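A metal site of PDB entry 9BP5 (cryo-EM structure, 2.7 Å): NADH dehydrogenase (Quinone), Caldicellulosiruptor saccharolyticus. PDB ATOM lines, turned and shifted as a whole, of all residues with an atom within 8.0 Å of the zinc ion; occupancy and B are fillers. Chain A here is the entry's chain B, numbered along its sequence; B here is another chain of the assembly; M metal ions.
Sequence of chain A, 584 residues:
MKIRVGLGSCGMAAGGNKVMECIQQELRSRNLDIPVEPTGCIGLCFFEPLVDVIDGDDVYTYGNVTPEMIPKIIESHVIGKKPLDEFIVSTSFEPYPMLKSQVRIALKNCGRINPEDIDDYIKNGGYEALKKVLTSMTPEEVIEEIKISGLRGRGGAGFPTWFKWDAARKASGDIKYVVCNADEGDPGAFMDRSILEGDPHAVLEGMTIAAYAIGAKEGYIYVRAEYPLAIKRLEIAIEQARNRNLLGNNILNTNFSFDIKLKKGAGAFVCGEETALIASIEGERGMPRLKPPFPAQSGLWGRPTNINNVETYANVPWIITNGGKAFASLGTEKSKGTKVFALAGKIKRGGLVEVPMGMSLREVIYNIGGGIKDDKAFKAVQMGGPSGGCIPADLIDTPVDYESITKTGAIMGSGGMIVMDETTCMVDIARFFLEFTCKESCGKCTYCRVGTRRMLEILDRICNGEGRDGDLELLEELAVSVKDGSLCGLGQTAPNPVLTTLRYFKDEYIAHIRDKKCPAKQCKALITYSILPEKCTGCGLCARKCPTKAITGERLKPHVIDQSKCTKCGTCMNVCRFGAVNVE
The zinc ion is bound by the side-chain carboxylate (OE2) of Glu 48 (2.0 Å), the side-chain sulfur (SG) of Cys 10 (2.3 Å), the side-chain sulfur (SG) of Cys 45 (2.3 Å) and the side-chain sulfur (SG) of Cys 41 (2.3 Å). The zinc ion has four donor atoms within binding distance.
SG of Cys 41 sits close to N of Gly 43, at 3.6 Å.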
ATOM      1  N   GLY A   6     -12.035 -25.409 -12.566  1.00  0.00           N
ATOM      2  CA  GLY A   6     -11.680 -25.934 -13.870  1.00  0.00           C
ATOM      3  C   GLY A   6     -10.284 -26.505 -13.898  1.00  0.00           C
ATOM      4  O   GLY A   6      -9.303 -25.788 -14.079  1.00  0.00           O
ATOM      5  N   LEU A   7     -10.188 -27.822 -13.706  1.00  0.00           N
ATOM      6  CA  LEU A   7      -8.915 -28.531 -13.665  1.00  0.00           C
ATOM      7  C   LEU A   7      -8.695 -29.272 -14.984  1.00  0.00           C
ATOM      8  O   LEU A   7      -8.869 -30.480 -15.091  1.00  0.00           O
ATOM      9  CB  LEU A   7      -8.879 -29.485 -12.480  1.00  0.00           C
ATOM     10  CG  LEU A   7      -8.965 -28.822 -11.109  1.00  0.00           C
ATOM     11  CD1 LEU A   7      -8.898 -29.875 -10.046  1.00  0.00           C
ATOM     12  CD2 LEU A   7      -7.844 -27.817 -10.949  1.00  0.00           C
ATOM     13  N   GLY A   8      -8.313 -28.516 -16.000  1.00  0.00           N
ATOM     14  CA  GLY A   8      -7.800 -29.083 -17.229  1.00  0.00           C
ATOM     15  C   GLY A   8      -6.303 -29.219 -17.172  1.00  0.00           C
ATOM     16  O   GLY A   8      -5.669 -29.072 -16.122  1.00  0.00           O
ATOM     17  N   SER A   9      -5.717 -29.520 -18.331  1.00  0.00           N
ATOM     18  CA  SER A   9      -4.258 -29.449 -18.435  1.00  0.00           C
ATOM     19  C   SER A   9      -3.784 -28.026 -18.203  1.00  0.00           C
ATOM     20  O   SER A   9      -2.758 -27.798 -17.541  1.00  0.00           O
ATOM     21  CB  SER A   9      -3.803 -29.957 -19.799  1.00  0.00           C
ATOM     22  OG  SER A   9      -2.614 -29.302 -20.219  1.00  0.00           O
ATOM     23  N   CYS A  10      -4.504 -27.038 -18.742  1.00  0.00           N
ATOM     24  CA  CYS A  10      -4.227 -25.642 -18.467  1.00  0.00           C
ATOM     25  C   CYS A  10      -4.779 -25.186 -17.123  1.00  0.00           C
ATOM     26  O   CYS A  10      -4.304 -24.168 -16.595  1.00  0.00           O
ATOM     27  CB  CYS A  10      -4.814 -24.766 -19.576  1.00  0.00           C
ATOM     28  SG  CYS A  10      -6.378 -25.374 -20.235  1.00  0.00           S
ATOM     29  N   GLY A  11      -5.765 -25.889 -16.571  1.00  0.00           N
ATOM     30  CA  GLY A  11      -6.319 -25.490 -15.285  1.00  0.00           C
ATOM     31  C   GLY A  11      -5.312 -25.587 -14.159  1.00  0.00           C
ATOM     32  O   GLY A  11      -5.153 -24.659 -13.368  1.00  0.00           O
ATOM     33  N   MET A  12      -4.608 -26.724 -14.069  1.00  0.00           N
ATOM     34  CA  MET A  12      -3.560 -26.860 -13.073  1.00  0.00           C
ATOM     35  C   MET A  12      -2.268 -26.152 -13.465  1.00  0.00           C
ATOM     36  O   MET A  12      -1.363 -26.047 -12.640  1.00  0.00           O
ATOM     37  CB  MET A  12      -3.269 -28.328 -12.779  1.00  0.00           C
ATOM     38  CG  MET A  12      -4.494 -29.208 -12.788  1.00  0.00           C
ATOM     39  SD  MET A  12      -4.218 -30.631 -11.728  1.00  0.00           S
ATOM     40  CE  MET A  12      -5.150 -31.895 -12.562  1.00  0.00           C
ATOM     41  N   ALA A  14      -2.435 -22.981 -14.332  1.00  0.00           N
ATOM     42  CA  ALA A  14      -2.704 -21.617 -13.934  1.00  0.00           C
ATOM     43  C   ALA A  14      -3.020 -21.490 -12.449  1.00  0.00           C
ATOM     44  O   ALA A  14      -3.515 -20.445 -12.017  1.00  0.00           O
ATOM     45  CB  ALA A  14      -3.856 -21.041 -14.768  1.00  0.00           C
ATOM     46  N   GLY A  40     -13.484 -29.816 -16.599  1.00  0.00           N
ATOM     47  CA  GLY A  40     -12.568 -29.630 -17.694  1.00  0.00           C
ATOM     48  C   GLY A  40     -12.430 -28.183 -18.103  1.00  0.00           C
ATOM     49  O   GLY A  40     -12.732 -27.258 -17.354  1.00  0.00           O
ATOM     50  N   CYS A  41     -11.976 -27.987 -19.342  1.00  0.00           N
ATOM     51  CA  CYS A  41     -11.779 -26.659 -19.899  1.00  0.00           C
ATOM     52  C   CYS A  41     -13.011 -26.255 -20.698  1.00  0.00           C
ATOM     53  O   CYS A  41     -13.377 -26.938 -21.666  1.00  0.00           O
ATOM     54  CB  CYS A  41     -10.534 -26.620 -20.776  1.00  0.00           C
ATOM     55  SG  CYS A  41     -10.067 -24.977 -21.373  1.00  0.00           S
ATOM     56  N   ILE A  42     -13.659 -25.158 -20.297  1.00  0.00           N
ATOM     57  CA  ILE A  42     -14.838 -24.678 -21.002  1.00  0.00           C
ATOM     58  C   ILE A  42     -14.480 -23.997 -22.317  1.00  0.00           C
ATOM     59  O   ILE A  42     -15.369 -23.748 -23.141  1.00  0.00           O
ATOM     60  CB  ILE A  42     -15.646 -23.720 -20.111  1.00  0.00           C
ATOM     61  CG1 ILE A  42     -17.075 -23.555 -20.629  1.00  0.00           C
ATOM     62  CG2 ILE A  42     -14.971 -22.370 -20.049  1.00  0.00           C
ATOM     63  CD1 ILE A  42     -17.846 -22.461 -19.945  1.00  0.00           C
ATOM     64  N   GLY A  43     -13.203 -23.720 -22.544  1.00  0.00           N
ATOM     65  CA  GLY A  43     -12.744 -23.027 -23.721  1.00  0.00           C
ATOM     66  C   GLY A  43     -12.206 -21.639 -23.451  1.00  0.00           C
ATOM     67  O   GLY A  43     -11.441 -21.112 -24.266  1.00  0.00           O
ATOM     68  N   LEU A  44     -12.568 -21.038 -22.321  1.00  0.00           N
ATOM     69  CA  LEU A  44     -12.038 -19.735 -21.914  1.00  0.00           C
ATOM     70  C   LEU A  44     -10.721 -19.961 -21.167  1.00  0.00           C
ATOM     71  O   LEU A  44     -10.591 -19.668 -19.979  1.00  0.00           O
ATOM     72  CB  LEU A  44     -13.047 -18.985 -21.069  1.00  0.00           C
ATOM     73  CG  LEU A  44     -14.498 -18.988 -21.556  1.00  0.00           C
ATOM     74  CD1 LEU A  44     -15.446 -18.684 -20.398  1.00  0.00           C
ATOM     75  CD2 LEU A  44     -14.686 -17.994 -22.671  1.00  0.00           C
ATOM     76  N   CYS A  45      -9.742 -20.488 -21.897  1.00  0.00           N
ATOM     77  CA  CYS A  45      -8.445 -20.799 -21.302  1.00  0.00           C
ATOM     78  C   CYS A  45      -7.668 -19.556 -20.900  1.00  0.00           C
ATOM     79  O   CYS A  45      -6.650 -19.674 -20.210  1.00  0.00           O
ATOM     80  CB  CYS A  45      -7.615 -21.652 -22.258  1.00  0.00           C
ATOM     81  SG  CYS A  45      -8.320 -23.280 -22.603  1.00  0.00           S
ATOM     82  N   PHE A  46      -8.100 -18.377 -21.324  1.00  0.00           N
ATOM     83  CA  PHE A  46      -7.480 -17.115 -20.930  1.00  0.00           C
ATOM     84  C   PHE A  46      -8.115 -16.532 -19.672  1.00  0.00           C
ATOM     85  O   PHE A  46      -7.768 -15.412 -19.291  1.00  0.00           O
ATOM     86  CB  PHE A  46      -7.561 -16.105 -22.074  1.00  0.00           C
ATOM     87  CG  PHE A  46      -8.958 -15.740 -22.465  1.00  0.00           C
ATOM     88  CD1 PHE A  46      -9.739 -16.603 -23.216  1.00  0.00           C
ATOM     89  CD2 PHE A  46      -9.493 -14.516 -22.110  1.00  0.00           C
ATOM     90  CE1 PHE A  46     -11.018 -16.269 -23.581  1.00  0.00           C
ATOM     91  CE2 PHE A  46     -10.767 -14.171 -22.471  1.00  0.00           C
ATOM     92  CZ  PHE A  46     -11.530 -15.052 -23.205  1.00  0.00           C
ATOM     93  N   PHE A  47      -9.045 -17.248 -19.044  1.00  0.00           N
ATOM     94  CA  PHE A  47      -9.663 -16.825 -17.794  1.00  0.00           C
ATOM     95  C   PHE A  47      -9.428 -17.807 -16.665  1.00  0.00           C
ATOM     96  O   PHE A  47     -10.026 -17.667 -15.595  1.00  0.00           O
ATOM     97  CB  PHE A  47     -11.174 -16.625 -17.993  1.00  0.00           C
ATOM     98  CG  PHE A  47     -11.542 -15.217 -18.367  1.00  0.00           C
ATOM     99  CD1 PHE A  47     -11.093 -14.152 -17.611  1.00  0.00           C
ATOM    100  CD2 PHE A  47     -12.337 -14.970 -19.465  1.00  0.00           C
ATOM    101  CE1 PHE A  47     -11.433 -12.861 -17.951  1.00  0.00           C
ATOM    102  CE2 PHE A  47     -12.674 -13.684 -19.819  1.00  0.00           C
ATOM    103  CZ  PHE A  47     -12.226 -12.628 -19.059  1.00  0.00           C
ATOM    104  N   GLU A  48      -8.562 -18.810 -16.867  1.00  0.00           N
ATOM    105  CA  GLU A  48      -8.294 -19.778 -15.826  1.00  0.00           C
ATOM    106  C   GLU A  48      -7.535 -19.127 -14.662  1.00  0.00           C
ATOM    107  O   GLU A  48      -6.721 -18.230 -14.870  1.00  0.00           O
ATOM    108  CB  GLU A  48      -7.493 -20.950 -16.375  1.00  0.00           C
ATOM    109  CG  GLU A  48      -7.947 -21.410 -17.745  1.00  0.00           C
ATOM    110  CD  GLU A  48      -8.777 -22.672 -17.685  1.00  0.00           C
ATOM    111  OE1 GLU A  48      -9.191 -23.055 -16.578  1.00  0.00           O
ATOM    112  OE2 GLU A  48      -9.014 -23.277 -18.748  1.00  0.00           O
ATOM    113  N   LEU A  50     -11.076 -21.049 -13.395  1.00  0.00           N
ATOM    114  CA  LEU A  50     -12.495 -20.718 -13.441  1.00  0.00           C
ATOM    115  C   LEU A  50     -13.222 -21.454 -12.329  1.00  0.00           C
ATOM    116  O   LEU A  50     -13.066 -22.662 -12.180  1.00  0.00           O
ATOM    117  CB  LEU A  50     -13.096 -21.080 -14.796  1.00  0.00           C
ATOM    118  CG  LEU A  50     -12.658 -20.249 -16.005  1.00  0.00           C
ATOM    119  CD1 LEU A  50     -13.081 -20.937 -17.292  1.00  0.00           C
ATOM    120  CD2 LEU A  50     -13.243 -18.863 -15.928  1.00  0.00           C
ATOM    121  N   PHE A 190      -4.259 -28.934 -28.743  1.00  0.00           N
ATOM    122  CA  PHE A 190      -4.600 -29.483 -27.435  1.00  0.00           C
ATOM    123  C   PHE A 190      -6.078 -29.842 -27.322  1.00  0.00           C
ATOM    124  O   PHE A 190      -6.594 -29.952 -26.198  1.00  0.00           O
ATOM    125  CB  PHE A 190      -4.232 -28.500 -26.331  1.00  0.00           C
ATOM    126  CG  PHE A 190      -4.620 -27.083 -26.607  1.00  0.00           C
ATOM    127  CD1 PHE A 190      -3.762 -26.226 -27.269  1.00  0.00           C
ATOM    128  CD2 PHE A 190      -5.850 -26.602 -26.201  1.00  0.00           C
ATOM    129  CE1 PHE A 190      -4.127 -24.928 -27.519  1.00  0.00           C
ATOM    130  CE2 PHE A 190      -6.215 -25.295 -26.454  1.00  0.00           C
ATOM    131  CZ  PHE A 190      -5.350 -24.459 -27.116  1.00  0.00           C
ATOM    132  N   SER A 194      -7.848 -31.877 -24.052  1.00  0.00           N
ATOM    133  CA  SER A 194      -8.913 -31.241 -23.289  1.00  0.00           C
ATOM    134  C   SER A 194     -10.197 -32.052 -23.324  1.00  0.00           C
ATOM    135  O   SER A 194     -10.931 -32.114 -22.335  1.00  0.00           O
ATOM    136  CB  SER A 194      -9.162 -29.824 -23.822  1.00  0.00           C
ATOM    137  OG  SER A 194      -8.049 -28.986 -23.553  1.00  0.00           O
ATOM    138  N   GLU A 197      -9.697 -34.853 -20.919  1.00  0.00           N
ATOM    139  CA  GLU A 197      -9.710 -34.355 -19.559  1.00  0.00           C
ATOM    140  C   GLU A 197     -11.062 -33.815 -19.120  1.00  0.00           C
ATOM    141  O   GLU A 197     -11.275 -33.620 -17.920  1.00  0.00           O
ATOM    142  CB  GLU A 197      -8.669 -33.249 -19.392  1.00  0.00           C
ATOM    143  CG  GLU A 197      -7.244 -33.749 -19.384  1.00  0.00           C
ATOM    144  CD  GLU A 197      -6.266 -32.698 -19.816  1.00  0.00           C
ATOM    145  OE1 GLU A 197      -6.664 -31.511 -19.881  1.00  0.00           O
ATOM    146  OE2 GLU A 197      -5.101 -33.038 -20.076  1.00  0.00           O
ATOM    147  N   GLY A 350      -7.575 -16.785 -26.811  1.00  0.00           N
ATOM    148  CA  GLY A 350      -7.226 -18.101 -27.312  1.00  0.00           C
ATOM    149  C   GLY A 350      -7.803 -19.220 -26.482  1.00  0.00           C
ATOM    150  O   GLY A 350      -8.213 -18.998 -25.339  1.00  0.00           O
ATOM    151  N   GLY A 351      -7.855 -20.419 -27.034  1.00  0.00           N
ATOM    152  CA  GLY A 351      -8.379 -21.565 -26.320  1.00  0.00           C
ATOM    153  C   GLY A 351      -9.143 -22.464 -27.260  1.00  0.00           C
ATOM    154  O   GLY A 351      -9.013 -22.385 -28.470  1.00  0.00           O
ATOM    155  N   LEU A 352      -9.957 -23.346 -26.672  1.00  0.00           N
ATOM    156  CA  LEU A 352     -10.752 -24.271 -27.459  1.00  0.00           C
ATOM    157  C   LEU A 352     -12.008 -23.583 -27.965  1.00  0.00           C
ATOM    158  O   LEU A 352     -12.737 -22.954 -27.183  1.00  0.00           O
ATOM    159  CB  LEU A 352     -11.128 -25.498 -26.630  1.00  0.00           C
ATOM    160  CG  LEU A 352     -10.213 -26.723 -26.688  1.00  0.00           C
ATOM    161  CD1 LEU A 352     -10.968 -27.936 -26.221  1.00  0.00           C
ATOM    162  CD2 LEU A 352      -9.678 -26.923 -28.084  1.00  0.00           C
ATOM    163  N   GLY B 139      -0.191 -27.741 -22.993  1.00  0.00           N
ATOM    164  CA  GLY B 139      -1.598 -27.524 -22.784  1.00  0.00           C
ATOM    165  C   GLY B 139      -1.966 -26.095 -22.434  1.00  0.00           C
ATOM    166  O   GLY B 139      -3.049 -25.639 -22.804  1.00  0.00           O
ATOM    167  N   CYS B 140      -1.079 -25.381 -21.745  1.00  0.00           N
ATOM    168  CA  CYS B 140      -1.340 -24.009 -21.318  1.00  0.00           C
ATOM    169  C   CYS B 140      -0.731 -23.052 -22.340  1.00  0.00           C
ATOM    170  O   CYS B 140       0.296 -22.431 -22.121  1.00  0.00           O
ATOM    171  CB  CYS B 140      -0.761 -23.772 -19.930  1.00  0.00           C
ATOM    172  SG  CYS B 140       0.856 -24.514 -19.672  1.00  0.00           S
ATOM    173  N   CYS B 141      -1.409 -22.942 -23.485  1.00  0.00           N
ATOM    174  CA  CYS B 141      -0.923 -22.059 -24.541  1.00  0.00           C
ATOM    175  C   CYS B 141      -1.100 -20.594 -24.170  1.00  0.00           C
ATOM    176  O   CYS B 141      -0.315 -19.753 -24.617  1.00  0.00           O
ATOM    177  CB  CYS B 141      -1.649 -22.358 -25.851  1.00  0.00           C
ATOM    178  SG  CYS B 141      -0.855 -23.587 -26.889  1.00  0.00           S
ATOM    179  N   SER B 142      -2.104 -20.272 -23.360  1.00  0.00           N
ATOM    180  CA  SER B 142      -2.387 -18.877 -23.036  1.00  0.00           C
ATOM    181  C   SER B 142      -1.326 -18.252 -22.147  1.00  0.00           C
ATOM    182  O   SER B 142      -1.310 -17.025 -22.011  1.00  0.00           O
ATOM    183  CB  SER B 142      -3.755 -18.757 -22.360  1.00  0.00           C
ATOM    184  OG  SER B 142      -4.354 -17.514 -22.672  1.00  0.00           O
HETATM  185 ZN    ZN M   1      -8.207 -24.003 -20.425  1.00  0.00          ZN
